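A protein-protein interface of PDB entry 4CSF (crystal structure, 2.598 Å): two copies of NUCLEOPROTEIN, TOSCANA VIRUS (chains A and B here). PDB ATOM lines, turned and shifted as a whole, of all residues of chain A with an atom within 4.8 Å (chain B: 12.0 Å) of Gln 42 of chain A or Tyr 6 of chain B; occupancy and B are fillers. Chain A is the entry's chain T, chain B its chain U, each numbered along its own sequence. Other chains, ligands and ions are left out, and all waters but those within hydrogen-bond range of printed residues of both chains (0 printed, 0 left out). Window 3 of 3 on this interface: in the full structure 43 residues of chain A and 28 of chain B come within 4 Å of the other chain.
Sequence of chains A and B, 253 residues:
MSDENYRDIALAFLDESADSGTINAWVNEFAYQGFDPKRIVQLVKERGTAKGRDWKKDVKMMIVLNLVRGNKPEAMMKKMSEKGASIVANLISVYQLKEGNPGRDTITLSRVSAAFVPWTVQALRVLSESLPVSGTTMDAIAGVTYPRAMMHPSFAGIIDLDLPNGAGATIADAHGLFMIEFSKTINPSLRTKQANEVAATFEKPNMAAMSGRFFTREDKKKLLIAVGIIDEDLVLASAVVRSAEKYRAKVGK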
ATOM      1  N   LYS A  38     -16.111   2.863 -23.046  1.00  0.00           N
ATOM      2  CA  LYS A  38     -17.289   2.410 -23.781  1.00  0.00           C
ATOM      3  C   LYS A  38     -17.072   1.018 -24.361  1.00  0.00           C
ATOM      4  O   LYS A  38     -17.922   0.136 -24.225  1.00  0.00           O
ATOM      5  CB  LYS A  38     -17.618   3.394 -24.905  1.00  0.00           C
ATOM      6  CG  LYS A  38     -18.744   2.941 -25.815  1.00  0.00           C
ATOM      7  CD  LYS A  38     -18.503   3.372 -27.257  1.00  0.00           C
ATOM      8  CE  LYS A  38     -18.346   4.883 -27.380  1.00  0.00           C
ATOM      9  NZ  LYS A  38     -18.070   5.302 -28.789  1.00  0.00           N
ATOM     10  N   ARG A  39     -15.920   0.830 -24.997  1.00  0.00           N
ATOM     11  CA  ARG A  39     -15.552  -0.450 -25.592  1.00  0.00           C
ATOM     12  C   ARG A  39     -15.387  -1.531 -24.516  1.00  0.00           C
ATOM     13  O   ARG A  39     -15.677  -2.709 -24.750  1.00  0.00           O
ATOM     14  CB  ARG A  39     -14.262  -0.289 -26.401  1.00  0.00           C
ATOM     15  CG  ARG A  39     -13.861  -1.503 -27.213  1.00  0.00           C
ATOM     16  CD  ARG A  39     -14.787  -1.741 -28.397  1.00  0.00           C
ATOM     17  NE  ARG A  39     -14.318  -2.860 -29.213  1.00  0.00           N
ATOM     18  CZ  ARG A  39     -15.109  -3.791 -29.737  1.00  0.00           C
ATOM     19  NH1 ARG A  39     -16.417  -3.739 -29.540  1.00  0.00           N
ATOM     20  NH2 ARG A  39     -14.586  -4.775 -30.460  1.00  0.00           N
ATOM     21  N   ILE A  40     -14.933  -1.120 -23.333  1.00  0.00           N
ATOM     22  CA  ILE A  40     -14.697  -2.047 -22.227  1.00  0.00           C
ATOM     23  C   ILE A  40     -15.992  -2.652 -21.690  1.00  0.00           C
ATOM     24  O   ILE A  40     -16.097  -3.875 -21.556  1.00  0.00           O
ATOM     25  CB  ILE A  40     -13.902  -1.393 -21.073  1.00  0.00           C
ATOM     26  CG1 ILE A  40     -12.486  -1.028 -21.529  1.00  0.00           C
ATOM     27  CG2 ILE A  40     -13.856  -2.325 -19.857  1.00  0.00           C
ATOM     28  CD1 ILE A  40     -11.662  -2.229 -21.977  1.00  0.00           C
ATOM     29  N   VAL A  41     -16.978  -1.810 -21.388  1.00  0.00           N
ATOM     30  CA  VAL A  41     -18.250  -2.327 -20.887  1.00  0.00           C
ATOM     31  C   VAL A  41     -18.967  -3.150 -21.960  1.00  0.00           C
ATOM     32  O   VAL A  41     -19.703  -4.086 -21.647  1.00  0.00           O
ATOM     33  CB  VAL A  41     -19.183  -1.216 -20.302  1.00  0.00           C
ATOM     34  CG1 VAL A  41     -18.401   0.033 -19.968  1.00  0.00           C
ATOM     35  CG2 VAL A  41     -20.322  -0.904 -21.243  1.00  0.00           C
ATOM     36  N   GLN A  42     -18.731  -2.810 -23.224  1.00  0.00           N
ATOM     37  CA  GLN A  42     -19.298  -3.565 -24.335  1.00  0.00           C
ATOM     38  C   GLN A  42     -18.757  -4.986 -24.364  1.00  0.00           C
ATOM     39  O   GLN A  42     -19.524  -5.955 -24.375  1.00  0.00           O
ATOM     40  CB  GLN A  42     -18.992  -2.881 -25.665  1.00  0.00           C
ATOM     41  CG  GLN A  42     -19.451  -3.683 -26.880  1.00  0.00           C
ATOM     42  CD  GLN A  42     -19.223  -2.961 -28.192  1.00  0.00           C
ATOM     43  OE1 GLN A  42     -18.493  -1.969 -28.258  1.00  0.00           O
ATOM     44  NE2 GLN A  42     -19.846  -3.461 -29.248  1.00  0.00           N
ATOM     45  N   LEU A  43     -17.430  -5.100 -24.373  1.00  0.00           N
ATOM     46  CA  LEU A  43     -16.757  -6.399 -24.432  1.00  0.00           C
ATOM     47  C   LEU A  43     -17.047  -7.263 -23.206  1.00  0.00           C
ATOM     48  O   LEU A  43     -17.181  -8.483 -23.317  1.00  0.00           O
ATOM     49  CB  LEU A  43     -15.247  -6.212 -24.624  1.00  0.00           C
ATOM     50  CG  LEU A  43     -14.848  -5.624 -25.984  1.00  0.00           C
ATOM     51  CD1 LEU A  43     -13.360  -5.336 -26.054  1.00  0.00           C
ATOM     52  CD2 LEU A  43     -15.266  -6.559 -27.107  1.00  0.00           C
ATOM     53  N   VAL A  44     -17.154  -6.627 -22.041  1.00  0.00           N
ATOM     54  CA  VAL A  44     -17.489  -7.341 -20.811  1.00  0.00           C
ATOM     55  C   VAL A  44     -18.875  -7.965 -20.912  1.00  0.00           C
ATOM     56  O   VAL A  44     -19.050  -9.153 -20.647  1.00  0.00           O
ATOM     57  CB  VAL A  44     -17.423  -6.421 -19.574  1.00  0.00           C
ATOM     58  CG1 VAL A  44     -18.115  -7.074 -18.392  1.00  0.00           C
ATOM     59  CG2 VAL A  44     -15.976  -6.092 -19.232  1.00  0.00           C
ATOM     60  N   LYS A  45     -19.853  -7.160 -21.312  1.00  0.00           N
ATOM     61  CA  LYS A  45     -21.225  -7.638 -21.447  1.00  0.00           C
ATOM     62  C   LYS A  45     -21.353  -8.703 -22.535  1.00  0.00           C
ATOM     63  O   LYS A  45     -22.031  -9.712 -22.339  1.00  0.00           O
ATOM     64  CB  LYS A  45     -22.183  -6.477 -21.726  1.00  0.00           C
ATOM     65  CG  LYS A  45     -23.642  -6.900 -21.810  1.00  0.00           C
ATOM     66  CD  LYS A  45     -24.522  -5.773 -22.320  1.00  0.00           C
ATOM     67  CE  LYS A  45     -25.959  -6.237 -22.494  1.00  0.00           C
ATOM     68  NZ  LYS A  45     -26.810  -5.170 -23.097  1.00  0.00           N
ATOM     69  N   GLU A  46     -20.695  -8.479 -23.671  1.00  0.00           N
ATOM     70  CA  GLU A  46     -20.743  -9.426 -24.784  1.00  0.00           C
ATOM     71  C   GLU A  46     -20.107 -10.770 -24.423  1.00  0.00           C
ATOM     72  O   GLU A  46     -20.743 -11.821 -24.547  1.00  0.00           O
ATOM     73  CB  GLU A  46     -20.072  -8.837 -26.029  1.00  0.00           C
ATOM     74  CG  GLU A  46     -20.884  -7.754 -26.731  1.00  0.00           C
ATOM     75  CD  GLU A  46     -20.157  -7.164 -27.927  1.00  0.00           C
ATOM     76  OE1 GLU A  46     -19.043  -7.638 -28.239  1.00  0.00           O
ATOM     77  OE2 GLU A  46     -20.699  -6.226 -28.554  1.00  0.00           O
ATOM     78  N   PHE A 214     -16.414  10.078 -21.480  1.00  0.00           N
ATOM     79  CA  PHE A 214     -17.326   8.943 -21.388  1.00  0.00           C
ATOM     80  C   PHE A 214     -18.524   9.336 -20.531  1.00  0.00           C
ATOM     81  O   PHE A 214     -19.676   9.121 -20.909  1.00  0.00           O
ATOM     82  CB  PHE A 214     -16.605   7.736 -20.784  1.00  0.00           C
ATOM     83  CG  PHE A 214     -17.469   6.502 -20.652  1.00  0.00           C
ATOM     84  CD1 PHE A 214     -18.129   5.968 -21.756  1.00  0.00           C
ATOM     85  CD2 PHE A 214     -17.595   5.855 -19.429  1.00  0.00           C
ATOM     86  CE1 PHE A 214     -18.916   4.819 -21.640  1.00  0.00           C
ATOM     87  CE2 PHE A 214     -18.382   4.706 -19.302  1.00  0.00           C
ATOM     88  CZ  PHE A 214     -19.042   4.190 -20.412  1.00  0.00           C
ATOM     89  N   ASN B   5     -26.218   4.115 -24.268  1.00  0.00           N
ATOM     90  CA  ASN B   5     -26.532   2.727 -23.926  1.00  0.00           C
ATOM     91  C   ASN B   5     -25.492   2.108 -22.984  1.00  0.00           C
ATOM     92  O   ASN B   5     -25.810   1.768 -21.843  1.00  0.00           O
ATOM     93  CB  ASN B   5     -26.701   1.880 -25.187  1.00  0.00           C
ATOM     94  N   TYR B   6     -24.258   1.960 -23.466  1.00  0.00           N
ATOM     95  CA  TYR B   6     -23.156   1.426 -22.656  1.00  0.00           C
ATOM     96  C   TYR B   6     -22.832   2.362 -21.492  1.00  0.00           C
ATOM     97  O   TYR B   6     -22.394   1.930 -20.425  1.00  0.00           O
ATOM     98  CB  TYR B   6     -21.913   1.192 -23.527  1.00  0.00           C
ATOM     99  CG  TYR B   6     -22.128   0.133 -24.587  1.00  0.00           C
ATOM    100  CD1 TYR B   6     -22.721  -1.084 -24.266  1.00  0.00           C
ATOM    101  CD2 TYR B   6     -21.751   0.347 -25.905  1.00  0.00           C
ATOM    102  CE1 TYR B   6     -22.934  -2.056 -25.226  1.00  0.00           C
ATOM    103  CE2 TYR B   6     -21.962  -0.621 -26.875  1.00  0.00           C
ATOM    104  CZ  TYR B   6     -22.553  -1.821 -26.529  1.00  0.00           C
ATOM    105  OH  TYR B   6     -22.768  -2.794 -27.479  1.00  0.00           O
ATOM    106  N   ARG B   7     -23.059   3.652 -21.710  1.00  0.00           N
ATOM    107  CA  ARG B   7     -22.863   4.649 -20.670  1.00  0.00           C
ATOM    108  C   ARG B   7     -23.868   4.437 -19.538  1.00  0.00           C
ATOM    109  O   ARG B   7     -23.510   4.490 -18.361  1.00  0.00           O
ATOM    110  CB  ARG B   7     -23.009   6.049 -21.268  1.00  0.00           C
ATOM    111  CG  ARG B   7     -22.572   7.173 -20.353  1.00  0.00           C
ATOM    112  CD  ARG B   7     -23.756   7.999 -19.889  1.00  0.00           C
ATOM    113  NE  ARG B   7     -24.477   8.620 -20.999  1.00  0.00           N
ATOM    114  CZ  ARG B   7     -25.509   9.446 -20.852  1.00  0.00           C
ATOM    115  NH1 ARG B   7     -25.948   9.761 -19.637  1.00  0.00           N
ATOM    116  NH2 ARG B   7     -26.103   9.962 -21.920  1.00  0.00           N
ATOM    117  N   ASP B   8     -25.123   4.185 -19.904  1.00  0.00           N
ATOM    118  CA  ASP B   8     -26.186   3.966 -18.927  1.00  0.00           C
ATOM    119  C   ASP B   8     -26.004   2.652 -18.167  1.00  0.00           C
ATOM    120  O   ASP B   8     -26.374   2.553 -16.996  1.00  0.00           O
ATOM    121  CB  ASP B   8     -27.560   4.013 -19.598  1.00  0.00           C
ATOM    122  CG  ASP B   8     -27.902   5.390 -20.126  1.00  0.00           C
ATOM    123  OD1 ASP B   8     -27.559   6.389 -19.456  1.00  0.00           O
ATOM    124  OD2 ASP B   8     -28.520   5.475 -21.211  1.00  0.00           O
ATOM    125  N   ILE B   9     -25.437   1.649 -18.835  1.00  0.00           N
ATOM    126  CA  ILE B   9     -25.122   0.373 -18.194  1.00  0.00           C
ATOM    127  C   ILE B   9     -24.125   0.578 -17.055  1.00  0.00           C
ATOM    128  O   ILE B   9     -24.337   0.106 -15.935  1.00  0.00           O
ATOM    129  CB  ILE B   9     -24.551  -0.654 -19.205  1.00  0.00           C
ATOM    130  CG1 ILE B   9     -25.643  -1.140 -20.160  1.00  0.00           C
ATOM    131  CG2 ILE B   9     -23.939  -1.838 -18.484  1.00  0.00           C
ATOM    132  CD1 ILE B   9     -25.131  -2.061 -21.248  1.00  0.00           C
ATOM    133  N   ALA B  10     -23.041   1.292 -17.348  1.00  0.00           N
ATOM    134  CA  ALA B  10     -22.022   1.595 -16.347  1.00  0.00           C
ATOM    135  C   ALA B  10     -22.607   2.430 -15.211  1.00  0.00           C
ATOM    136  O   ALA B  10     -22.345   2.179 -14.033  1.00  0.00           O
ATOM    137  CB  ALA B  10     -20.857   2.324 -16.990  1.00  0.00           C
ATOM    138  N   LEU B  11     -23.410   3.417 -15.586  1.00  0.00           N
ATOM    139  CA  LEU B  11     -24.029   4.329 -14.639  1.00  0.00           C
ATOM    140  C   LEU B  11     -24.993   3.618 -13.690  1.00  0.00           C
ATOM    141  O   LEU B  11     -25.193   4.057 -12.553  1.00  0.00           O
ATOM    142  CB  LEU B  11     -24.751   5.433 -15.411  1.00  0.00           C
ATOM    143  CG  LEU B  11     -24.337   6.894 -15.180  1.00  0.00           C
ATOM    144  CD1 LEU B  11     -22.920   7.065 -14.635  1.00  0.00           C
ATOM    145  CD2 LEU B  11     -24.569   7.769 -16.414  1.00  0.00           C
ATOM    146  N   ALA B  12     -25.585   2.520 -14.155  1.00  0.00           N
ATOM    147  CA  ALA B  12     -26.538   1.756 -13.345  1.00  0.00           C
ATOM    148  C   ALA B  12     -25.859   0.970 -12.217  1.00  0.00           C
ATOM    149  O   ALA B  12     -26.518   0.529 -11.273  1.00  0.00           O
ATOM    150  CB  ALA B  12     -27.354   0.821 -14.227  1.00  0.00           C
ATOM    151  N   PHE B  13     -24.541   0.811 -12.313  1.00  0.00           N
ATOM    152  CA  PHE B  13     -23.787   0.111 -11.280  1.00  0.00           C
ATOM    153  C   PHE B  13     -23.708   0.921  -9.993  1.00  0.00           C
ATOM    154  O   PHE B  13     -23.296   0.410  -8.958  1.00  0.00           O
ATOM    155  CB  PHE B  13     -22.391  -0.262 -11.782  1.00  0.00           C
ATOM    156  CG  PHE B  13     -22.336  -1.599 -12.455  1.00  0.00           C
ATOM    157  CD1 PHE B  13     -22.737  -1.743 -13.775  1.00  0.00           C
ATOM    158  CD2 PHE B  13     -21.896  -2.721 -11.764  1.00  0.00           C
ATOM    159  CE1 PHE B  13     -22.699  -2.986 -14.397  1.00  0.00           C
ATOM    160  CE2 PHE B  13     -21.854  -3.964 -12.379  1.00  0.00           C
ATOM    161  CZ  PHE B  13     -22.256  -4.093 -13.699  1.00  0.00           C
ATOM    162  N   LEU B  14     -24.099   2.189 -10.073  1.00  0.00           N
ATOM    163  CA  LEU B  14     -24.224   3.038  -8.895  1.00  0.00           C
ATOM    164  C   LEU B  14     -25.243   2.428  -7.940  1.00  0.00           C
ATOM    165  O   LEU B  14     -25.046   2.402  -6.724  1.00  0.00           O
ATOM    166  CB  LEU B  14     -24.699   4.431  -9.308  1.00  0.00           C
ATOM    167  CG  LEU B  14     -24.223   5.661  -8.520  1.00  0.00           C
ATOM    168  CD1 LEU B  14     -25.282   6.771  -8.426  1.00  0.00           C
ATOM    169  CD2 LEU B  14     -23.598   5.342  -7.157  1.00  0.00           C
ATOM    170  N   GLU B  16     -26.215  -0.677  -8.113  1.00  0.00           N
ATOM    171  CA  GLU B  16     -25.984  -2.113  -8.019  1.00  0.00           C
ATOM    172  C   GLU B  16     -25.433  -2.453  -6.636  1.00  0.00           C
ATOM    173  O   GLU B  16     -24.718  -1.651  -6.033  1.00  0.00           O
ATOM    174  CB  GLU B  16     -25.033  -2.579  -9.120  1.00  0.00           C
ATOM    175  CG  GLU B  16     -25.104  -4.072  -9.416  1.00  0.00           C
ATOM    176  CD  GLU B  16     -26.231  -4.459 -10.356  1.00  0.00           C
ATOM    177  OE1 GLU B  16     -26.478  -3.723 -11.337  1.00  0.00           O
ATOM    178  OE2 GLU B  16     -26.856  -5.515 -10.126  1.00  0.00           O
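The side-chain hydroxyl of Tyr 6 of chain B sits at hydrogen-bond distance from the side-chain amide nitrogen of Gln 42 of chain A (3.5 Å).
The side-chain amide oxygen of Gln 42 of chain A sits at hydrogen-bond distance from the guanidinium group of Arg 39 of chain A (3.0 Å). NE2 of Gln 42 of chain A is in hydrogen-bond range of OE2 of Glu 46 of chain A (3.0 Å). NH1 of Arg 7 of chain B lies within salt-bridge range of OD1 of Asp 8 of chain B, at 3.7 Å.
Among the printed residues, pairs that only touch across the chains: Lys 38 of chain A with Tyr 6 of chain B, Val 41 of chain A with Tyr 6 of chain B, Lys 45 of chain A with Ile 9 of chain B and Phe 214 of chain A with Arg 7 of chain B.
Of chain B, only Tyr 6 (3.97 Å) comes within 4 Å of Lys 38 of chain A. Of chain B, only Tyr 6 (3.5 Å) comes within 4 Å of Val 41 of chain A. Gln 42 of chain A touches just one residue of chain B: Tyr 6. No residue of chain B comes within 4 Å of Leu 43 of chain A. No residue of chain B comes within 4 Å of Glu 46 of chain A. Of the printed residues of chain B, Phe 214 of chain A touches Arg 7. Tyr 6 of chain B touches just these residues of chain A: Lys 38, Val 41 and Gln 42. Printed residues of chain A within 4 Å of Arg 7 of chain B: Phe 214. Of the printed residues of chain A, Ile 9 of chain B touches Lys 45. Leu 11 of chain B touches none of the printed residues of chain A. Phe 13 of chain B touches none of the printed residues of chain A.
Of the 10 printed residues of chain A, 5 touch a printed residue of chain B. Printed residues of chain A that touch a printed residue of chain B: Lys 38, Val 41, Gln 42, Lys 45 and Phe 214. Along chain A the printed residues that touch a printed residue of chain B span positions 38 to 214. Among the printed residues, 5 pairs touch across the chains.
No position is printed for both chains. Of the 5 pairs that touch across the chains among the printed residues, none has its exchanged pair printed and touching as well.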
